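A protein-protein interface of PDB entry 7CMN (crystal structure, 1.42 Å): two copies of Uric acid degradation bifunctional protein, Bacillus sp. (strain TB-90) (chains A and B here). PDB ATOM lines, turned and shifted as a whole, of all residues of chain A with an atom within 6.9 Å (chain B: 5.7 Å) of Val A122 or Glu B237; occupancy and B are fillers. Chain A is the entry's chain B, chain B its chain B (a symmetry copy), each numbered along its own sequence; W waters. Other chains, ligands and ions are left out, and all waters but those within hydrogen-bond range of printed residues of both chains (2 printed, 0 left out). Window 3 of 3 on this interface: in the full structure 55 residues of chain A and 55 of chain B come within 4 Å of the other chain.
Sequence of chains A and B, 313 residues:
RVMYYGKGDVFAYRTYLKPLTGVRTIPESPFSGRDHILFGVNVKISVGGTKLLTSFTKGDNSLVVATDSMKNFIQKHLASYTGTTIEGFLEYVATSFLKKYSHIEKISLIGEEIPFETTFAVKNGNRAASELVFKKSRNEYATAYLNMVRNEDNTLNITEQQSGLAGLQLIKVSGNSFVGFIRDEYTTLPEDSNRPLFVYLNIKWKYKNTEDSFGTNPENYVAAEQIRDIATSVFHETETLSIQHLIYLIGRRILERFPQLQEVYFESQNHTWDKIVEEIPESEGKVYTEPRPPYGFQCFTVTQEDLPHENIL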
ATOM      1  N   PHE A 120      15.745  19.536  14.940  1.00  0.00           N
ATOM      2  CA  PHE A 120      15.133  20.156  16.092  1.00  0.00           C
ATOM      3  C   PHE A 120      14.414  21.446  15.704  1.00  0.00           C
ATOM      4  O   PHE A 120      14.904  22.211  14.871  1.00  0.00           O
ATOM      5  CB  PHE A 120      16.173  20.501  17.177  1.00  0.00           C
ATOM      6  CG  PHE A 120      16.791  19.328  17.820  1.00  0.00           C
ATOM      7  CD1 PHE A 120      16.086  18.522  18.705  1.00  0.00           C
ATOM      8  CD2 PHE A 120      18.116  19.029  17.571  1.00  0.00           C
ATOM      9  CE1 PHE A 120      16.713  17.400  19.287  1.00  0.00           C
ATOM     10  CE2 PHE A 120      18.737  17.911  18.149  1.00  0.00           C
ATOM     11  CZ  PHE A 120      18.023  17.117  19.018  1.00  0.00           C
ATOM     12  N   ALA A 121      13.262  21.693  16.327  1.00  0.00           N
ATOM     13  CA  ALA A 121      12.610  22.983  16.237  1.00  0.00           C
ATOM     14  C   ALA A 121      11.906  23.327  17.538  1.00  0.00           C
ATOM     15  O   ALA A 121      11.359  22.456  18.220  1.00  0.00           O
ATOM     16  CB  ALA A 121      11.597  22.977  15.082  1.00  0.00           C
ATOM     17  N   VAL A 122      11.892  24.607  17.867  1.00  0.00           N
ATOM     18  CA  VAL A 122      11.143  25.094  19.017  1.00  0.00           C
ATOM     19  C   VAL A 122       9.745  25.450  18.539  1.00  0.00           C
ATOM     20  O   VAL A 122       9.569  25.956  17.434  1.00  0.00           O
ATOM     21  CB  VAL A 122      11.859  26.284  19.682  1.00  0.00           C
ATOM     22  CG1 VAL A 122      10.967  26.901  20.748  1.00  0.00           C
ATOM     23  CG2 VAL A 122      13.172  25.844  20.290  1.00  0.00           C
ATOM     24  N   LYS A 123       8.728  25.153  19.353  1.00  0.00           N
ATOM     25  CA  LYS A 123       7.358  25.527  19.037  1.00  0.00           C
ATOM     26  C   LYS A 123       6.477  25.255  20.242  1.00  0.00           C
ATOM     27  O   LYS A 123       6.636  24.230  20.914  1.00  0.00           O
ATOM     28  CB  LYS A 123       6.831  24.733  17.839  1.00  0.00           C
ATOM     29  N   ASN A 124       5.546  26.172  20.503  1.00  0.00           N
ATOM     30  CA  ASN A 124       4.553  26.030  21.572  1.00  0.00           C
ATOM     31  C   ASN A 124       5.179  25.812  22.951  1.00  0.00           C
ATOM     32  O   ASN A 124       4.517  25.285  23.861  1.00  0.00           O
ATOM     33  CB  ASN A 124       3.542  24.916  21.263  1.00  0.00           C
ATOM     34  N   GLY A 125       6.443  26.209  23.135  1.00  0.00           N
ATOM     35  CA  GLY A 125       7.083  26.192  24.436  1.00  0.00           C
ATOM     36  C   GLY A 125       8.189  25.159  24.579  1.00  0.00           C
ATOM     37  O   GLY A 125       9.008  25.283  25.495  1.00  0.00           O
ATOM     38  N   ASN A 126       8.227  24.148  23.712  1.00  0.00           N
ATOM     39  CA  ASN A 126       9.225  23.096  23.825  1.00  0.00           C
ATOM     40  C   ASN A 126       9.984  22.941  22.512  1.00  0.00           C
ATOM     41  O   ASN A 126       9.553  23.393  21.448  1.00  0.00           O
ATOM     42  CB  ASN A 126       8.558  21.753  24.158  1.00  0.00           C
ATOM     43  CG  ASN A 126       7.377  21.460  23.250  1.00  0.00           C
ATOM     44  OD1 ASN A 126       6.588  22.351  22.957  1.00  0.00           O
ATOM     45  ND2 ASN A 126       7.247  20.220  22.823  1.00  0.00           N
ATOM     46  N   ARG A 127      11.136  22.283  22.598  1.00  0.00           N
ATOM     47  CA  ARG A 127      11.928  21.880  21.443  1.00  0.00           C
ATOM     48  C   ARG A 127      11.652  20.402  21.184  1.00  0.00           C
ATOM     49  O   ARG A 127      11.643  19.598  22.121  1.00  0.00           O
ATOM     50  CB  ARG A 127      13.420  22.056  21.735  1.00  0.00           C
ATOM     51  CG  ARG A 127      14.319  21.601  20.608  1.00  0.00           C
ATOM     52  CD  ARG A 127      15.805  21.779  20.952  1.00  0.00           C
ATOM     53  NE  ARG A 127      16.176  20.965  22.087  1.00  0.00           N
ATOM     54  CZ  ARG A 127      16.561  21.421  23.272  1.00  0.00           C
ATOM     55  NH1 ARG A 127      16.643  22.717  23.544  1.00  0.00           N
ATOM     56  NH2 ARG A 127      16.879  20.556  24.240  1.00  0.00           N
ATOM     57  N   ALA A 128      11.415  20.043  19.927  1.00  0.00           N
ATOM     58  CA  ALA A 128      11.146  18.652  19.590  1.00  0.00           C
ATOM     59  C   ALA A 128      11.483  18.441  18.129  1.00  0.00           C
ATOM     60  O   ALA A 128      11.744  19.391  17.382  1.00  0.00           O
ATOM     61  CB  ALA A 128       9.690  18.289  19.880  1.00  0.00           C
ATOM     62  N   LEU A 132       8.243  18.585   9.757  1.00  0.00           N
ATOM     63  CA  LEU A 132       8.278  19.270   8.457  1.00  0.00           C
ATOM     64  C   LEU A 132       9.674  19.356   7.846  1.00  0.00           C
ATOM     65  O   LEU A 132       9.813  19.255   6.604  1.00  0.00           O
ATOM     66  CB  LEU A 132       7.776  20.689   8.564  1.00  0.00           C
ATOM     67  CG  LEU A 132       6.344  20.838   9.049  1.00  0.00           C
ATOM     68  CD1 LEU A 132       5.954  22.328   9.186  1.00  0.00           C
ATOM     69  CD2 LEU A 132       5.353  20.157   8.113  1.00  0.00           C
ATOM     70  N   VAL A 133      10.702  19.641   8.659  1.00  0.00           N
ATOM     71  CA  VAL A 133      12.058  19.921   8.205  1.00  0.00           C
ATOM     72  C   VAL A 133      12.931  18.695   8.435  1.00  0.00           C
ATOM     73  O   VAL A 133      13.110  18.242   9.593  1.00  0.00           O
ATOM     74  CB  VAL A 133      12.644  21.146   8.924  1.00  0.00           C
ATOM     75  CG1 VAL A 133      14.028  21.417   8.425  1.00  0.00           C
ATOM     76  CG2 VAL A 133      11.751  22.350   8.781  1.00  0.00           C
ATOM     77  N   PRO B  27      17.799  27.972  23.457  1.00  0.00           N
ATOM     78  CA  PRO B  27      16.541  27.190  23.375  1.00  0.00           C
ATOM     79  C   PRO B  27      16.479  26.262  22.198  1.00  0.00           C
ATOM     80  O   PRO B  27      15.868  25.193  22.273  1.00  0.00           O
ATOM     81  CB  PRO B  27      15.458  28.275  23.322  1.00  0.00           C
ATOM     82  CG  PRO B  27      16.073  29.480  23.979  1.00  0.00           C
ATOM     83  CD  PRO B  27      17.561  29.414  23.654  1.00  0.00           C
ATOM     84  N   GLU B  28      17.123  26.626  21.080  1.00  0.00           N
ATOM     85  CA  GLU B  28      16.979  25.840  19.874  1.00  0.00           C
ATOM     86  C   GLU B  28      17.803  24.560  19.872  1.00  0.00           C
ATOM     87  O   GLU B  28      17.598  23.718  18.987  1.00  0.00           O
ATOM     88  CB  GLU B  28      17.345  26.689  18.620  1.00  0.00           C
ATOM     89  CG  GLU B  28      16.342  27.802  18.279  1.00  0.00           C
ATOM     90  CD  GLU B  28      16.446  29.074  19.125  1.00  0.00           C
ATOM     91  OE1 GLU B  28      17.395  29.188  19.952  1.00  0.00           O
ATOM     92  OE2 GLU B  28      15.570  29.953  18.965  1.00  0.00           O
ATOM     93  N   LYS B 172      12.054  21.126   3.665  1.00  0.00           N
ATOM     94  CA  LYS B 172      10.844  21.315   4.442  1.00  0.00           C
ATOM     95  C   LYS B 172       9.662  21.001   3.528  1.00  0.00           C
ATOM     96  O   LYS B 172       9.480  21.673   2.511  1.00  0.00           O
ATOM     97  CB  LYS B 172      10.746  22.764   4.960  1.00  0.00           C
ATOM     98  CG  LYS B 172       9.538  23.026   5.811  1.00  0.00           C
ATOM     99  CD  LYS B 172       9.425  24.486   6.270  1.00  0.00           C
ATOM    100  CE  LYS B 172       8.183  24.700   7.152  1.00  0.00           C
ATOM    101  NZ  LYS B 172       7.873  26.124   7.429  1.00  0.00           N
ATOM    102  N   ILE B 230      19.555  26.235  15.232  1.00  0.00           N
ATOM    103  CA  ILE B 230      18.844  27.471  14.934  1.00  0.00           C
ATOM    104  C   ILE B 230      18.273  27.426  13.513  1.00  0.00           C
ATOM    105  O   ILE B 230      17.124  27.789  13.272  1.00  0.00           O
ATOM    106  CB  ILE B 230      19.741  28.703  15.123  1.00  0.00           C
ATOM    107  CG1 ILE B 230      20.056  28.878  16.629  1.00  0.00           C
ATOM    108  CG2 ILE B 230      19.081  29.946  14.507  1.00  0.00           C
ATOM    109  CD1 ILE B 230      21.030  29.989  16.931  1.00  0.00           C
ATOM    110  N   THR B 232      17.502  24.898  11.565  1.00  0.00           N
ATOM    111  CA  THR B 232      16.379  23.988  11.406  1.00  0.00           C
ATOM    112  C   THR B 232      15.149  24.518  12.122  1.00  0.00           C
ATOM    113  O   THR B 232      14.026  24.442  11.604  1.00  0.00           O
ATOM    114  CB  THR B 232      16.731  22.566  11.829  1.00  0.00           C
ATOM    115  OG1 THR B 232      17.022  22.528  13.213  1.00  0.00           O
ATOM    116  CG2 THR B 232      17.899  22.047  11.016  1.00  0.00           C
ATOM    117  N   SER B 233      15.326  25.133  13.285  1.00  0.00           N
ATOM    118  CA  SER B 233      14.188  25.625  14.030  1.00  0.00           C
ATOM    119  C   SER B 233      13.524  26.774  13.288  1.00  0.00           C
ATOM    120  O   SER B 233      12.301  26.774  13.080  1.00  0.00           O
ATOM    121  CB  SER B 233      14.604  26.065  15.447  1.00  0.00           C
ATOM    122  OG  SER B 233      13.447  26.336  16.192  1.00  0.00           O
ATOM    123  N   VAL B 234      14.321  27.739  12.833  1.00  0.00           N
ATOM    124  CA  VAL B 234      13.736  28.873  12.104  1.00  0.00           C
ATOM    125  C   VAL B 234      13.041  28.402  10.825  1.00  0.00           C
ATOM    126  O   VAL B 234      11.959  28.874  10.490  1.00  0.00           O
ATOM    127  CB  VAL B 234      14.827  29.919  11.829  1.00  0.00           C
ATOM    128  CG1 VAL B 234      14.269  31.029  10.942  1.00  0.00           C
ATOM    129  CG2 VAL B 234      15.366  30.502  13.171  1.00  0.00           C
ATOM    130  N   PHE B 235      13.634  27.429  10.123  1.00  0.00           N
ATOM    131  CA  PHE B 235      13.002  26.916   8.888  1.00  0.00           C
ATOM    132  C   PHE B 235      11.635  26.337   9.226  1.00  0.00           C
ATOM    133  O   PHE B 235      10.625  26.619   8.565  1.00  0.00           O
ATOM    134  CB  PHE B 235      13.922  25.866   8.270  1.00  0.00           C
ATOM    135  CG  PHE B 235      13.687  25.546   6.805  1.00  0.00           C
ATOM    136  CD1 PHE B 235      12.740  26.210   6.062  1.00  0.00           C
ATOM    137  CD2 PHE B 235      14.468  24.567   6.201  1.00  0.00           C
ATOM    138  CE1 PHE B 235      12.573  25.904   4.690  1.00  0.00           C
ATOM    139  CE2 PHE B 235      14.314  24.243   4.872  1.00  0.00           C
ATOM    140  CZ  PHE B 235      13.376  24.905   4.115  1.00  0.00           C
ATOM    141  N   HIS B 236      11.577  25.535  10.295  1.00  0.00           N
ATOM    142  CA  HIS B 236      10.316  24.966  10.732  1.00  0.00           C
ATOM    143  C   HIS B 236       9.314  26.043  11.110  1.00  0.00           C
ATOM    144  O   HIS B 236       8.131  26.012  10.689  1.00  0.00           O
ATOM    145  CB  HIS B 236      10.583  24.081  11.964  1.00  0.00           C
ATOM    146  CG  HIS B 236       9.349  23.488  12.519  1.00  0.00           C
ATOM    147  ND1 HIS B 236       8.509  24.158  13.393  1.00  0.00           N
ATOM    148  CD2 HIS B 236       8.787  22.287  12.307  1.00  0.00           C
ATOM    149  CE1 HIS B 236       7.462  23.401  13.664  1.00  0.00           C
ATOM    150  NE2 HIS B 236       7.615  22.257  13.027  1.00  0.00           N
ATOM    151  N   GLU B 237       9.758  27.036  11.898  1.00  0.00           N
ATOM    152  CA  GLU B 237       8.852  28.047  12.441  1.00  0.00           C
ATOM    153  C   GLU B 237       8.243  28.952  11.363  1.00  0.00           C
ATOM    154  O   GLU B 237       7.187  29.497  11.600  1.00  0.00           O
ATOM    155  CB  GLU B 237       9.619  28.942  13.435  1.00  0.00           C
ATOM    156  CG  GLU B 237      10.095  28.250  14.702  1.00  0.00           C
ATOM    157  CD  GLU B 237      11.017  29.142  15.541  1.00  0.00           C
ATOM    158  OE1 GLU B 237      10.548  30.221  15.947  1.00  0.00           O
ATOM    159  OE2 GLU B 237      12.206  28.802  15.758  1.00  0.00           O
ATOM    160  N   THR B 238       8.930  29.136  10.247  1.00  0.00           N
ATOM    161  CA  THR B 238       8.669  30.206   9.288  1.00  0.00           C
ATOM    162  C   THR B 238       7.826  29.701   8.125  1.00  0.00           C
ATOM    163  O   THR B 238       8.166  28.710   7.489  1.00  0.00           O
ATOM    164  CB  THR B 238       9.994  30.738   8.717  1.00  0.00           C
ATOM    165  OG1 THR B 238      10.872  31.181   9.768  1.00  0.00           O
ATOM    166  CG2 THR B 238       9.762  31.911   7.776  1.00  0.00           C
ATOM    167  N   GLU B 239       6.745  30.411   7.823  1.00  0.00           N
ATOM    168  CA  GLU B 239       6.077  30.232   6.541  1.00  0.00           C
ATOM    169  C   GLU B 239       6.940  30.981   5.541  1.00  0.00           C
ATOM    170  O   GLU B 239       6.795  32.185   5.339  1.00  0.00           O
ATOM    171  CB  GLU B 239       4.668  30.781   6.611  1.00  0.00           C
ATOM    172  CG  GLU B 239       3.837  30.181   7.731  1.00  0.00           C
ATOM    173  CD  GLU B 239       3.584  28.705   7.512  1.00  0.00           C
ATOM    174  OE1 GLU B 239       3.791  27.915   8.459  1.00  0.00           O
ATOM    175  OE2 GLU B 239       3.190  28.341   6.381  1.00  0.00           O
ATOM    176  N   ARG B 253      17.967  35.397  14.102  1.00  0.00           N
ATOM    177  CA  ARG B 253      17.912  34.554  15.293  1.00  0.00           C
ATOM    178  C   ARG B 253      19.326  34.264  15.815  1.00  0.00           C
ATOM    179  O   ARG B 253      19.578  34.309  17.034  1.00  0.00           O
ATOM    180  CB  ARG B 253      17.168  33.245  14.979  1.00  0.00           C
ATOM    181  CG  ARG B 253      16.945  32.344  16.205  1.00  0.00           C
ATOM    182  CD  ARG B 253      15.909  32.911  17.153  1.00  0.00           C
ATOM    183  NE  ARG B 253      14.608  33.035  16.500  1.00  0.00           N
ATOM    184  CZ  ARG B 253      13.739  32.042  16.335  1.00  0.00           C
ATOM    185  NH1 ARG B 253      14.022  30.806  16.782  1.00  0.00           N
ATOM    186  NH2 ARG B 253      12.617  32.273  15.661  1.00  0.00           N
HETATM  187  O   HOH W   1      15.332  23.615  17.580  1.00  0.00           O
HETATM  188  O   HOH W   2      18.456  20.410  14.118  1.00  0.00           O
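N of Ala A121 sits at hydrogen-bond distance from O of Ala A128 (3.0 Å). The side-chain carboxylate (OE2) of Glu B28 is in salt-bridge range of the guanidinium group (NH1) of Arg B253, at 2.8 Å. The side-chain amino group (NZ) of Lys B172 lies within hydrogen-bond range of the backbone carbonyl oxygen (O) of Phe B235, 3.0 Å away. NZ of Lys B172 is in hydrogen-bond range of O of His B236 (3.3 Å). The side-chain amino group (NZ) of Lys B172 sits at hydrogen-bond distance from the backbone carbonyl oxygen (O) of Thr B238 (2.6 Å). The side-chain carboxylate (OE2) of Glu B237 lies within hydrogen-bond range of the side-chain hydroxyl (OG) of Ser B233.
O of Phe A120 sits at hydrogen-bond distance from OG1 of Thr B232 (2.7 Å). The backbone carbonyl oxygen of Phe A120 sits at hydrogen-bond distance from the backbone NH of Ser B233, at 3.4 Å. N of Val A122 is in hydrogen-bond range of OG of Ser B233 (2.9 Å). The guanidinium group (NH1) of Arg A127 is in hydrogen-bond range of the backbone carbonyl oxygen (O) of Pro B27 (2.9 Å).
Of the 11 printed residues of chain A, 6 touch a printed residue of chain B. Hydrophobic or aromatic side chains of chain A within 4 Å of the printed part of chain B: Phe A120, Ala A121, Val A122, Leu A132 and Val A133. Of the 13 printed residues of chain B, 8 touch a printed residue of chain A. Printed residues of chain B that touch a printed residue of chain A: Pro B27, Glu B28, Lys B172, Thr B232, Ser B233, Phe B235, His B236 and Glu B237. Hydrophobic or aromatic side chains of chain B within 4 Å of the printed part of chain A: Phe B235 and His B236. Along chain B the printed residues that touch a printed residue of chain A span positions 27 to 237. Among the printed residues, no Asp or Glu carboxylate lies within 4 Å of a Lys or Arg side-chain nitrogen of the other chain.
Water W1 lies within hydrogen-bond range of O of Glu B28, O of Phe A120 and N of Ala A121. Water W2 bridges the side-chain hydroxyl of Thr B232 (2.7 Å) and the backbone NH of Phe A120 (3.0 Å).
No position is printed for both chains. Of the 15 pairs that touch across the chains among the printed residues, none has its exchanged pair printed and touching as well.
Among the printed residues, pairs that only touch across the chains: Leu A132 with Lys B172 (3.2 Å), Arg A127 with Glu B28 (3.3 Å), Val A122 with Pro B27 (3.4 Å), Ala A121 with His B236 (3.4 Å), Ala A121 with Ser B233 (3.5 Å), Val A133 with His B236 (3.5 Å), Val A122 with Glu B237 (3.6 Å), Val A133 with Lys B172 (3.8 Å), Val A122 with Glu B28 (3.8 Å), Val A133 with Phe B235 (3.9 Å) and Phe A120 with Glu B28 (3.96 Å).
Of the printed residues of chain B, Ala A121 touches Ser B233 (3.5 Å) and His B236 (3.4 Å). Of the printed residues of chain B, Val A122 touches Pro B27, Glu B28, Ser B233 and Glu B237. Asn A126 touches none of the printed residues of chain B. Printed residues of chain B within 4 Å of Val A133: Lys B172 (3.8 Å), Phe B235 (3.9 Å) and His B236 (3.5 Å). Glu B237 touches just one residue of chain A: Val A122. Arg B253 touches none of the printed residues of chain A. The nearest residue of chain A that does not touch Glu B237 is Ala A121 (5.5 Å). The nearest printed residue of chain A that does not touch Phe B235 is Leu A132 (6.4 Å).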
